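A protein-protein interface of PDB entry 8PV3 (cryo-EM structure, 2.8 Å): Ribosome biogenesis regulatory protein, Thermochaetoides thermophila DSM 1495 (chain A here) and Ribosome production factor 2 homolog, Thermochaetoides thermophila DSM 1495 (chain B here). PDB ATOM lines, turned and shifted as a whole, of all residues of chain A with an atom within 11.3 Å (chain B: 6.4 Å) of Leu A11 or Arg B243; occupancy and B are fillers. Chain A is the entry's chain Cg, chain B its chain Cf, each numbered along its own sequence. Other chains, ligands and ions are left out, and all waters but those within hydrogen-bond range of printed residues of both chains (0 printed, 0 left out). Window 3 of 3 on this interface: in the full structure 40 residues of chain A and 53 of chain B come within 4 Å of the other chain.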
ATOM      1  N   LEU A  11      16.224  23.976  24.355  1.00  0.00           N
ATOM      2  CA  LEU A  11      16.057  23.982  22.906  1.00  0.00           C
ATOM      3  C   LEU A  11      16.121  22.561  22.338  1.00  0.00           C
ATOM      4  O   LEU A  11      16.983  21.769  22.718  1.00  0.00           O
ATOM      5  CB  LEU A  11      17.097  24.917  22.266  1.00  0.00           C
ATOM      6  CG  LEU A  11      18.613  24.724  22.413  1.00  0.00           C
ATOM      7  CD1 LEU A  11      19.207  23.762  21.400  1.00  0.00           C
ATOM      8  CD2 LEU A  11      19.316  26.074  22.340  1.00  0.00           C
ATOM      9  N   PRO A  12      15.187  22.237  21.444  1.00  0.00           N
ATOM     10  CA  PRO A  12      15.027  20.845  21.015  1.00  0.00           C
ATOM     11  C   PRO A  12      16.104  20.398  20.042  1.00  0.00           C
ATOM     12  O   PRO A  12      16.751  21.206  19.371  1.00  0.00           O
ATOM     13  CB  PRO A  12      13.650  20.845  20.343  1.00  0.00           C
ATOM     14  CG  PRO A  12      13.520  22.231  19.812  1.00  0.00           C
ATOM     15  CD  PRO A  12      14.168  23.116  20.844  1.00  0.00           C
ATOM     16  N   VAL A  13      16.286  19.083  19.974  1.00  0.00           N
ATOM     17  CA  VAL A  13      17.137  18.446  18.979  1.00  0.00           C
ATOM     18  C   VAL A  13      16.313  17.579  18.030  1.00  0.00           C
ATOM     19  O   VAL A  13      16.869  16.812  17.247  1.00  0.00           O
ATOM     20  CB  VAL A  13      18.259  17.632  19.641  1.00  0.00           C
ATOM     21  CG1 VAL A  13      19.237  18.557  20.330  1.00  0.00           C
ATOM     22  CG2 VAL A  13      17.677  16.633  20.625  1.00  0.00           C
ATOM     23  N   THR A  14      14.990  17.692  18.093  1.00  0.00           N
ATOM     24  CA  THR A  14      14.088  16.946  17.232  1.00  0.00           C
ATOM     25  C   THR A  14      13.150  17.916  16.534  1.00  0.00           C
ATOM     26  O   THR A  14      12.584  18.816  17.161  1.00  0.00           O
ATOM     27  CB  THR A  14      13.275  15.914  18.027  1.00  0.00           C
ATOM     28  OG1 THR A  14      14.144  15.204  18.917  1.00  0.00           O
ATOM     29  CG2 THR A  14      12.603  14.924  17.089  1.00  0.00           C
ATOM     30  N   VAL A  15      12.988  17.729  15.227  1.00  0.00           N
ATOM     31  CA  VAL A  15      12.153  18.598  14.409  1.00  0.00           C
ATOM     32  C   VAL A  15      10.922  17.820  13.969  1.00  0.00           C
ATOM     33  O   VAL A  15      10.920  16.585  13.977  1.00  0.00           O
ATOM     34  CB  VAL A  15      12.923  19.146  13.189  1.00  0.00           C
ATOM     35  CG1 VAL A  15      14.109  19.976  13.646  1.00  0.00           C
ATOM     36  CG2 VAL A  15      13.373  18.013  12.290  1.00  0.00           C
ATOM     37  N   GLU A  16       9.873  18.549  13.599  1.00  0.00           N
ATOM     38  CA  GLU A  16       8.610  17.962  13.174  1.00  0.00           C
ATOM     39  C   GLU A  16       8.260  18.499  11.795  1.00  0.00           C
ATOM     40  O   GLU A  16       8.311  19.712  11.565  1.00  0.00           O
ATOM     41  CB  GLU A  16       7.497  18.271  14.186  1.00  0.00           C
ATOM     42  CG  GLU A  16       6.180  17.514  13.977  1.00  0.00           C
ATOM     43  CD  GLU A  16       5.261  18.166  12.956  1.00  0.00           C
ATOM     44  OE1 GLU A  16       5.326  19.403  12.801  1.00  0.00           O
ATOM     45  OE2 GLU A  16       4.478  17.438  12.310  1.00  0.00           O
ATOM     46  N   GLN A  49      19.385  32.359   4.997  1.00  0.00           N
ATOM     47  CA  GLN A  49      18.978  31.980   6.348  1.00  0.00           C
ATOM     48  C   GLN A  49      17.959  30.846   6.318  1.00  0.00           C
ATOM     49  O   GLN A  49      18.061  29.887   7.093  1.00  0.00           O
ATOM     50  CB  GLN A  49      18.423  33.199   7.086  1.00  0.00           C
ATOM     51  CG  GLN A  49      18.187  33.004   8.583  1.00  0.00           C
ATOM     52  CD  GLN A  49      16.813  32.444   8.907  1.00  0.00           C
ATOM     53  OE1 GLN A  49      15.851  32.669   8.175  1.00  0.00           O
ATOM     54  NE2 GLN A  49      16.719  31.709  10.008  1.00  0.00           N
ATOM     55  N   ALA A  52      19.780  27.739   5.229  1.00  0.00           N
ATOM     56  CA  ALA A  52      20.587  27.217   6.324  1.00  0.00           C
ATOM     57  C   ALA A  52      19.720  26.547   7.380  1.00  0.00           C
ATOM     58  O   ALA A  52      20.151  25.585   8.018  1.00  0.00           O
ATOM     59  CB  ALA A  52      21.417  28.339   6.945  1.00  0.00           C
ATOM     60  N   SER A  53      18.497  27.046   7.585  1.00  0.00           N
ATOM     61  CA  SER A  53      17.575  26.378   8.503  1.00  0.00           C
ATOM     62  C   SER A  53      17.182  24.997   7.990  1.00  0.00           C
ATOM     63  O   SER A  53      17.157  24.024   8.760  1.00  0.00           O
ATOM     64  CB  SER A  53      16.334  27.242   8.719  1.00  0.00           C
ATOM     65  OG  SER A  53      15.590  27.366   7.520  1.00  0.00           O
ATOM     66  N   VAL A  54      16.889  24.891   6.689  1.00  0.00           N
ATOM     67  CA  VAL A  54      16.573  23.589   6.094  1.00  0.00           C
ATOM     68  C   VAL A  54      17.774  22.650   6.183  1.00  0.00           C
ATOM     69  O   VAL A  54      17.635  21.459   6.507  1.00  0.00           O
ATOM     70  CB  VAL A  54      16.096  23.770   4.641  1.00  0.00           C
ATOM     71  CG1 VAL A  54      15.811  22.425   3.997  1.00  0.00           C
ATOM     72  CG2 VAL A  54      14.852  24.634   4.604  1.00  0.00           C
ATOM     73  N   ALA A  55      18.972  23.177   5.911  1.00  0.00           N
ATOM     74  CA  ALA A  55      20.192  22.384   6.007  1.00  0.00           C
ATOM     75  C   ALA A  55      20.450  21.913   7.431  1.00  0.00           C
ATOM     76  O   ALA A  55      20.888  20.777   7.646  1.00  0.00           O
ATOM     77  CB  ALA A  55      21.376  23.203   5.509  1.00  0.00           C
ATOM     78  N   ARG A  56      20.204  22.784   8.413  1.00  0.00           N
ATOM     79  CA  ARG A  56      20.376  22.414   9.810  1.00  0.00           C
ATOM     80  C   ARG A  56      19.408  21.314  10.210  1.00  0.00           C
ATOM     81  O   ARG A  56      19.783  20.383  10.928  1.00  0.00           O
ATOM     82  CB  ARG A  56      20.185  23.641  10.700  1.00  0.00           C
ATOM     83  CG  ARG A  56      20.770  23.492  12.086  1.00  0.00           C
ATOM     84  CD  ARG A  56      19.847  24.077  13.139  1.00  0.00           C
ATOM     85  NE  ARG A  56      18.654  23.260  13.331  1.00  0.00           N
ATOM     86  CZ  ARG A  56      18.608  22.163  14.073  1.00  0.00           C
ATOM     87  NH1 ARG A  56      19.671  21.721  14.723  1.00  0.00           N
ATOM     88  NH2 ARG A  56      17.463  21.492  14.169  1.00  0.00           N
ATOM     89  N   ASP A  57      18.159  21.401   9.742  1.00  0.00           N
ATOM     90  CA  ASP A  57      17.180  20.356  10.034  1.00  0.00           C
ATOM     91  C   ASP A  57      17.604  19.019   9.435  1.00  0.00           C
ATOM     92  O   ASP A  57      17.536  17.975  10.100  1.00  0.00           O
ATOM     93  CB  ASP A  57      15.807  20.770   9.507  1.00  0.00           C
ATOM     94  CG  ASP A  57      15.214  21.932  10.277  1.00  0.00           C
ATOM     95  OD1 ASP A  57      15.526  22.071  11.478  1.00  0.00           O
ATOM     96  OD2 ASP A  57      14.439  22.709   9.681  1.00  0.00           O
ATOM     97  N   GLY A  58      18.064  19.040   8.179  1.00  0.00           N
ATOM     98  CA  GLY A  58      18.497  17.805   7.536  1.00  0.00           C
ATOM     99  C   GLY A  58      19.723  17.194   8.190  1.00  0.00           C
ATOM    100  O   GLY A  58      19.784  15.978   8.404  1.00  0.00           O
ATOM    101  N   ALA A  59      20.708  18.029   8.530  1.00  0.00           N
ATOM    102  CA  ALA A  59      21.895  17.537   9.220  1.00  0.00           C
ATOM    103  C   ALA A  59      21.546  16.998  10.599  1.00  0.00           C
ATOM    104  O   ALA A  59      22.107  15.985  11.034  1.00  0.00           O
ATOM    105  CB  ALA A  59      22.936  18.649   9.326  1.00  0.00           C
ATOM    106  N   GLN A  60      20.604  17.648  11.289  1.00  0.00           N
ATOM    107  CA  GLN A  60      20.190  17.193  12.610  1.00  0.00           C
ATOM    108  C   GLN A  60      19.544  15.817  12.544  1.00  0.00           C
ATOM    109  O   GLN A  60      19.905  14.920  13.313  1.00  0.00           O
ATOM    110  CB  GLN A  60      19.231  18.209  13.231  1.00  0.00           C
ATOM    111  CG  GLN A  60      18.706  17.812  14.592  1.00  0.00           C
ATOM    112  CD  GLN A  60      19.724  18.029  15.687  1.00  0.00           C
ATOM    113  OE1 GLN A  60      20.233  19.135  15.863  1.00  0.00           O
ATOM    114  NE2 GLN A  60      20.028  16.973  16.430  1.00  0.00           N
ATOM    115  N   VAL A  61      18.607  15.619  11.610  1.00  0.00           N
ATOM    116  CA  VAL A  61      17.936  14.321  11.546  1.00  0.00           C
ATOM    117  C   VAL A  61      18.893  13.240  11.053  1.00  0.00           C
ATOM    118  O   VAL A  61      18.804  12.083  11.480  1.00  0.00           O
ATOM    119  CB  VAL A  61      16.651  14.382  10.694  1.00  0.00           C
ATOM    120  CG1 VAL A  61      15.598  15.217  11.392  1.00  0.00           C
ATOM    121  CG2 VAL A  61      16.913  14.891   9.295  1.00  0.00           C
ATOM    122  N   LEU A  62      19.846  13.598  10.185  1.00  0.00           N
ATOM    123  CA  LEU A  62      20.815  12.609   9.717  1.00  0.00           C
ATOM    124  C   LEU A  62      21.755  12.180  10.839  1.00  0.00           C
ATOM    125  O   LEU A  62      22.053  10.988  10.992  1.00  0.00           O
ATOM    126  CB  LEU A  62      21.603  13.168   8.533  1.00  0.00           C
ATOM    127  CG  LEU A  62      22.466  12.172   7.759  1.00  0.00           C
ATOM    128  CD1 LEU A  62      21.699  10.893   7.472  1.00  0.00           C
ATOM    129  CD2 LEU A  62      22.933  12.805   6.471  1.00  0.00           C
ATOM    130  N   ILE A  63      22.219  13.139  11.647  1.00  0.00           N
ATOM    131  CA  ILE A  63      23.083  12.817  12.781  1.00  0.00           C
ATOM    132  C   ILE A  63      22.325  11.987  13.810  1.00  0.00           C
ATOM    133  O   ILE A  63      22.867  11.026  14.371  1.00  0.00           O
ATOM    134  CB  ILE A  63      23.662  14.111  13.389  1.00  0.00           C
ATOM    135  CG1 ILE A  63      24.730  14.694  12.464  1.00  0.00           C
ATOM    136  CG2 ILE A  63      24.255  13.867  14.770  1.00  0.00           C
ATOM    137  CD1 ILE A  63      25.898  13.771  12.230  1.00  0.00           C
ATOM    138  N   ASN A  64      21.054  12.329  14.056  1.00  0.00           N
ATOM    139  CA  ASN A  64      20.243  11.555  14.994  1.00  0.00           C
ATOM    140  C   ASN A  64      20.049  10.122  14.514  1.00  0.00           C
ATOM    141  O   ASN A  64      20.178   9.176  15.301  1.00  0.00           O
ATOM    142  CB  ASN A  64      18.888  12.231  15.195  1.00  0.00           C
ATOM    143  CG  ASN A  64      19.002  13.582  15.868  1.00  0.00           C
ATOM    144  OD1 ASN A  64      20.030  13.909  16.461  1.00  0.00           O
ATOM    145  ND2 ASN A  64      17.944  14.378  15.779  1.00  0.00           N
ATOM    146  N   LEU A  67      23.386   8.204  14.848  1.00  0.00           N
ATOM    147  CA  LEU A  67      23.753   7.919  16.227  1.00  0.00           C
ATOM    148  C   LEU A  67      22.760   7.014  16.943  1.00  0.00           C
ATOM    149  O   LEU A  67      23.100   6.472  17.999  1.00  0.00           O
ATOM    150  CB  LEU A  67      23.908   9.222  17.013  1.00  0.00           C
ATOM    151  CG  LEU A  67      25.124  10.078  16.661  1.00  0.00           C
ATOM    152  CD1 LEU A  67      25.207  11.284  17.577  1.00  0.00           C
ATOM    153  CD2 LEU A  67      26.400   9.260  16.736  1.00  0.00           C
ATOM    154  N   ARG B 233      28.622  21.943  13.118  1.00  0.00           N
ATOM    155  CA  ARG B 233      29.085  22.093  14.487  1.00  0.00           C
ATOM    156  C   ARG B 233      28.042  21.519  15.433  1.00  0.00           C
ATOM    157  O   ARG B 233      26.836  21.667  15.215  1.00  0.00           O
ATOM    158  CB  ARG B 233      29.352  23.560  14.839  1.00  0.00           C
ATOM    159  CG  ARG B 233      30.458  24.208  14.029  1.00  0.00           C
ATOM    160  CD  ARG B 233      30.647  25.663  14.423  1.00  0.00           C
ATOM    161  NE  ARG B 233      29.495  26.482  14.065  1.00  0.00           N
ATOM    162  CZ  ARG B 233      28.682  27.055  14.941  1.00  0.00           C
ATOM    163  NH1 ARG B 233      28.865  26.918  16.244  1.00  0.00           N
ATOM    164  NH2 ARG B 233      27.661  27.783  14.500  1.00  0.00           N
ATOM    165  N   THR B 234      28.512  20.860  16.488  1.00  0.00           N
ATOM    166  CA  THR B 234      27.643  20.196  17.447  1.00  0.00           C
ATOM    167  C   THR B 234      27.829  20.803  18.830  1.00  0.00           C
ATOM    168  O   THR B 234      28.943  21.170  19.213  1.00  0.00           O
ATOM    169  CB  THR B 234      27.919  18.695  17.497  1.00  0.00           C
ATOM    170  OG1 THR B 234      29.307  18.472  17.769  1.00  0.00           O
ATOM    171  CG2 THR B 234      27.554  18.051  16.173  1.00  0.00           C
ATOM    172  N   LYS B 235      26.728  20.904  19.574  1.00  0.00           N
ATOM    173  CA  LYS B 235      26.717  21.505  20.897  1.00  0.00           C
ATOM    174  C   LYS B 235      25.951  20.611  21.863  1.00  0.00           C
ATOM    175  O   LYS B 235      25.143  19.773  21.457  1.00  0.00           O
ATOM    176  CB  LYS B 235      26.084  22.902  20.880  1.00  0.00           C
ATOM    177  CG  LYS B 235      26.846  23.932  20.068  1.00  0.00           C
ATOM    178  CD  LYS B 235      26.163  25.285  20.124  1.00  0.00           C
ATOM    179  CE  LYS B 235      26.842  26.279  19.202  1.00  0.00           C
ATOM    180  NZ  LYS B 235      28.205  26.635  19.680  1.00  0.00           N
ATOM    181  N   ARG B 236      26.223  20.797  23.153  1.00  0.00           N
ATOM    182  CA  ARG B 236      25.480  20.091  24.188  1.00  0.00           C
ATOM    183  C   ARG B 236      24.050  20.610  24.253  1.00  0.00           C
ATOM    184  O   ARG B 236      23.802  21.805  24.061  1.00  0.00           O
ATOM    185  CB  ARG B 236      26.159  20.260  25.546  1.00  0.00           C
ATOM    186  CG  ARG B 236      27.607  19.821  25.583  1.00  0.00           C
ATOM    187  CD  ARG B 236      28.167  19.864  26.993  1.00  0.00           C
ATOM    188  NE  ARG B 236      29.536  19.364  27.047  1.00  0.00           N
ATOM    189  CZ  ARG B 236      29.860  18.087  27.196  1.00  0.00           C
ATOM    190  NH1 ARG B 236      28.936  17.147  27.313  1.00  0.00           N
ATOM    191  NH2 ARG B 236      31.144  17.744  27.227  1.00  0.00           N
ATOM    192  N   SER B 237      23.107  19.710  24.522  1.00  0.00           N
ATOM    193  CA  SER B 237      21.703  20.074  24.648  1.00  0.00           C
ATOM    194  C   SER B 237      21.054  19.477  25.889  1.00  0.00           C
ATOM    195  O   SER B 237      19.828  19.558  26.034  1.00  0.00           O
ATOM    196  CB  SER B 237      20.931  19.649  23.397  1.00  0.00           C
ATOM    197  OG  SER B 237      20.823  18.239  23.323  1.00  0.00           O
ATOM    198  N   LEU B 241      21.639  13.043  22.562  1.00  0.00           N
ATOM    199  CA  LEU B 241      21.844  13.426  21.173  1.00  0.00           C
ATOM    200  C   LEU B 241      22.269  14.893  21.084  1.00  0.00           C
ATOM    201  O   LEU B 241      21.661  15.756  21.723  1.00  0.00           O
ATOM    202  CB  LEU B 241      20.565  13.185  20.368  1.00  0.00           C
ATOM    203  CG  LEU B 241      20.209  11.752  19.935  1.00  0.00           C
ATOM    204  CD1 LEU B 241      19.753  10.846  21.085  1.00  0.00           C
ATOM    205  CD2 LEU B 241      19.141  11.800  18.856  1.00  0.00           C
ATOM    206  N   PRO B 242      23.303  15.206  20.305  1.00  0.00           N
ATOM    207  CA  PRO B 242      23.809  16.580  20.252  1.00  0.00           C
ATOM    208  C   PRO B 242      22.940  17.491  19.397  1.00  0.00           C
ATOM    209  O   PRO B 242      22.093  17.051  18.619  1.00  0.00           O
ATOM    210  CB  PRO B 242      25.199  16.418  19.628  1.00  0.00           C
ATOM    211  CG  PRO B 242      25.066  15.220  18.767  1.00  0.00           C
ATOM    212  CD  PRO B 242      24.111  14.292  19.478  1.00  0.00           C
ATOM    213  N   ARG B 243      23.179  18.790  19.555  1.00  0.00           N
ATOM    214  CA  ARG B 243      22.466  19.816  18.804  1.00  0.00           C
ATOM    215  C   ARG B 243      23.334  20.274  17.638  1.00  0.00           C
ATOM    216  O   ARG B 243      24.445  20.773  17.843  1.00  0.00           O
ATOM    217  CB  ARG B 243      22.105  20.991  19.710  1.00  0.00           C
ATOM    218  CG  ARG B 243      21.775  22.280  18.980  1.00  0.00           C
ATOM    219  CD  ARG B 243      20.405  22.205  18.333  1.00  0.00           C
ATOM    220  NE  ARG B 243      20.060  23.449  17.657  1.00  0.00           N
ATOM    221  CZ  ARG B 243      18.869  23.717  17.141  1.00  0.00           C
ATOM    222  NH1 ARG B 243      17.874  22.848  17.212  1.00  0.00           N
ATOM    223  NH2 ARG B 243      18.671  24.885  16.539  1.00  0.00           N
ATOM    224  N   VAL B 244      22.824  20.112  16.422  1.00  0.00           N
ATOM    225  CA  VAL B 244      23.592  20.398  15.216  1.00  0.00           C
ATOM    226  C   VAL B 244      23.383  21.848  14.804  1.00  0.00           C
ATOM    227  O   VAL B 244      22.250  22.340  14.752  1.00  0.00           O
ATOM    228  CB  VAL B 244      23.190  19.429  14.089  1.00  0.00           C
ATOM    229  CG1 VAL B 244      23.867  19.801  12.783  1.00  0.00           C
ATOM    230  CG2 VAL B 244      23.532  18.002  14.474  1.00  0.00           C
ATOM    231  N   GLU B 245      24.485  22.544  14.527  1.00  0.00           N
ATOM    232  CA  GLU B 245      24.449  23.888  13.969  1.00  0.00           C
ATOM    233  C   GLU B 245      25.327  23.925  12.727  1.00  0.00           C
ATOM    234  O   GLU B 245      26.390  23.300  12.684  1.00  0.00           O
ATOM    235  CB  GLU B 245      24.919  24.938  14.984  1.00  0.00           C
ATOM    236  CG  GLU B 245      24.044  25.039  16.222  1.00  0.00           C
ATOM    237  CD  GLU B 245      22.698  25.680  15.939  1.00  0.00           C
ATOM    238  OE1 GLU B 245      22.590  26.439  14.952  1.00  0.00           O
ATOM    239  OE2 GLU B 245      21.745  25.421  16.703  1.00  0.00           O
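The side-chain amide nitrogen of Gln A60 sits at hydrogen-bond distance from the backbone carbonyl oxygen of Pro B242, at 3.0 Å. The guanidinium group of Arg B243 sits at hydrogen-bond distance from the backbone carbonyl oxygen of Pro A12, 2.9 Å away. The backbone carbonyl oxygen (O) of Val B244 is in hydrogen-bond range of the guanidinium group (NH1) of Arg A56, 2.7 Å away. OE1 of Gln A60 lies within hydrogen-bond range of N of Val B244 (2.8 Å). NH1 of Arg A56 sits close to NH1 of Arg B243.
OG of Ser B237 lies within hydrogen-bond range of O of Leu B241. The side-chain carboxylate (OE2) of Glu B245 is in salt-bridge range of the guanidinium group (NE) of Arg B243. NE2 of Gln A60 lies within hydrogen-bond range of O of Val A13 (3.3 Å). The backbone carbonyl oxygen of Val A13 lies within hydrogen-bond range of the side-chain amide nitrogen of Asn A64 (3.0 Å). NH2 of Arg A56 lies within salt-bridge range of OD1 of Asp A57. The side-chain amide oxygen (OE1) of Gln A60 is in hydrogen-bond range of the guanidinium group (NH1) of Arg A56, 2.9 Å away.
Leu A11 touches Arg B243. Val A13 touches Ser B237. CG1 of Val A13 touches O of Leu B241, at 3.96 Å. Pro B242 touches Val A13. CA of Arg B243 touches CG1 of Val A13 (3.8 Å). Val B244 touches Ala A59 (CG1 to CB, 3.8 Å). OE1 of Gln A60 touches C of Arg B243, at 3.8 Å. CD2 of Leu B241 touches OD1 of Asn A64, 3.3 Å away. CD1 of Leu A67 touches CD of Pro B242, at 3.7 Å.
Of chain B, only Arg B243 (3.6 Å) comes within 4 Å of Leu A11. Printed residues of chain B within 4 Å of Gln A60: Pro B242 (3.0 Å), Arg B243 (3.8 Å) and Val B244 (2.8 Å). Leu A62 touches none of the printed residues of chain B. Printed residues of chain B within 4 Å of Asn A64: Leu B241 (3.3 Å). Arg B233 touches none of the printed residues of chain A. No residue of chain A comes within 4 Å of Thr B234. No residue of chain A comes within 4 Å of Lys B235. Arg B243 touches five residues of chain A. Val B244 touches three residues of chain A. No residue of chain A comes within 4 Å of Glu B245. The nearest residue of chain B that does not touch Leu A11 is Ser B237 (4.5 Å). The nearest residue of chain A that does not touch Arg B243 is Val A15 (5.9 Å).
Printed residues of chain B that touch a printed residue of chain A: Ser B237, Leu B241, Pro B242, Arg B243 and Val B244. Hydrophobic or aromatic side chains of chain A within 4 Å of the printed part of chain B: Leu A11, Val A13, Ala A59 and Leu A67. Among the printed residues, no Asp or Glu carboxylate lies within 4 Å of a Lys or Arg side-chain nitrogen of the other chain.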
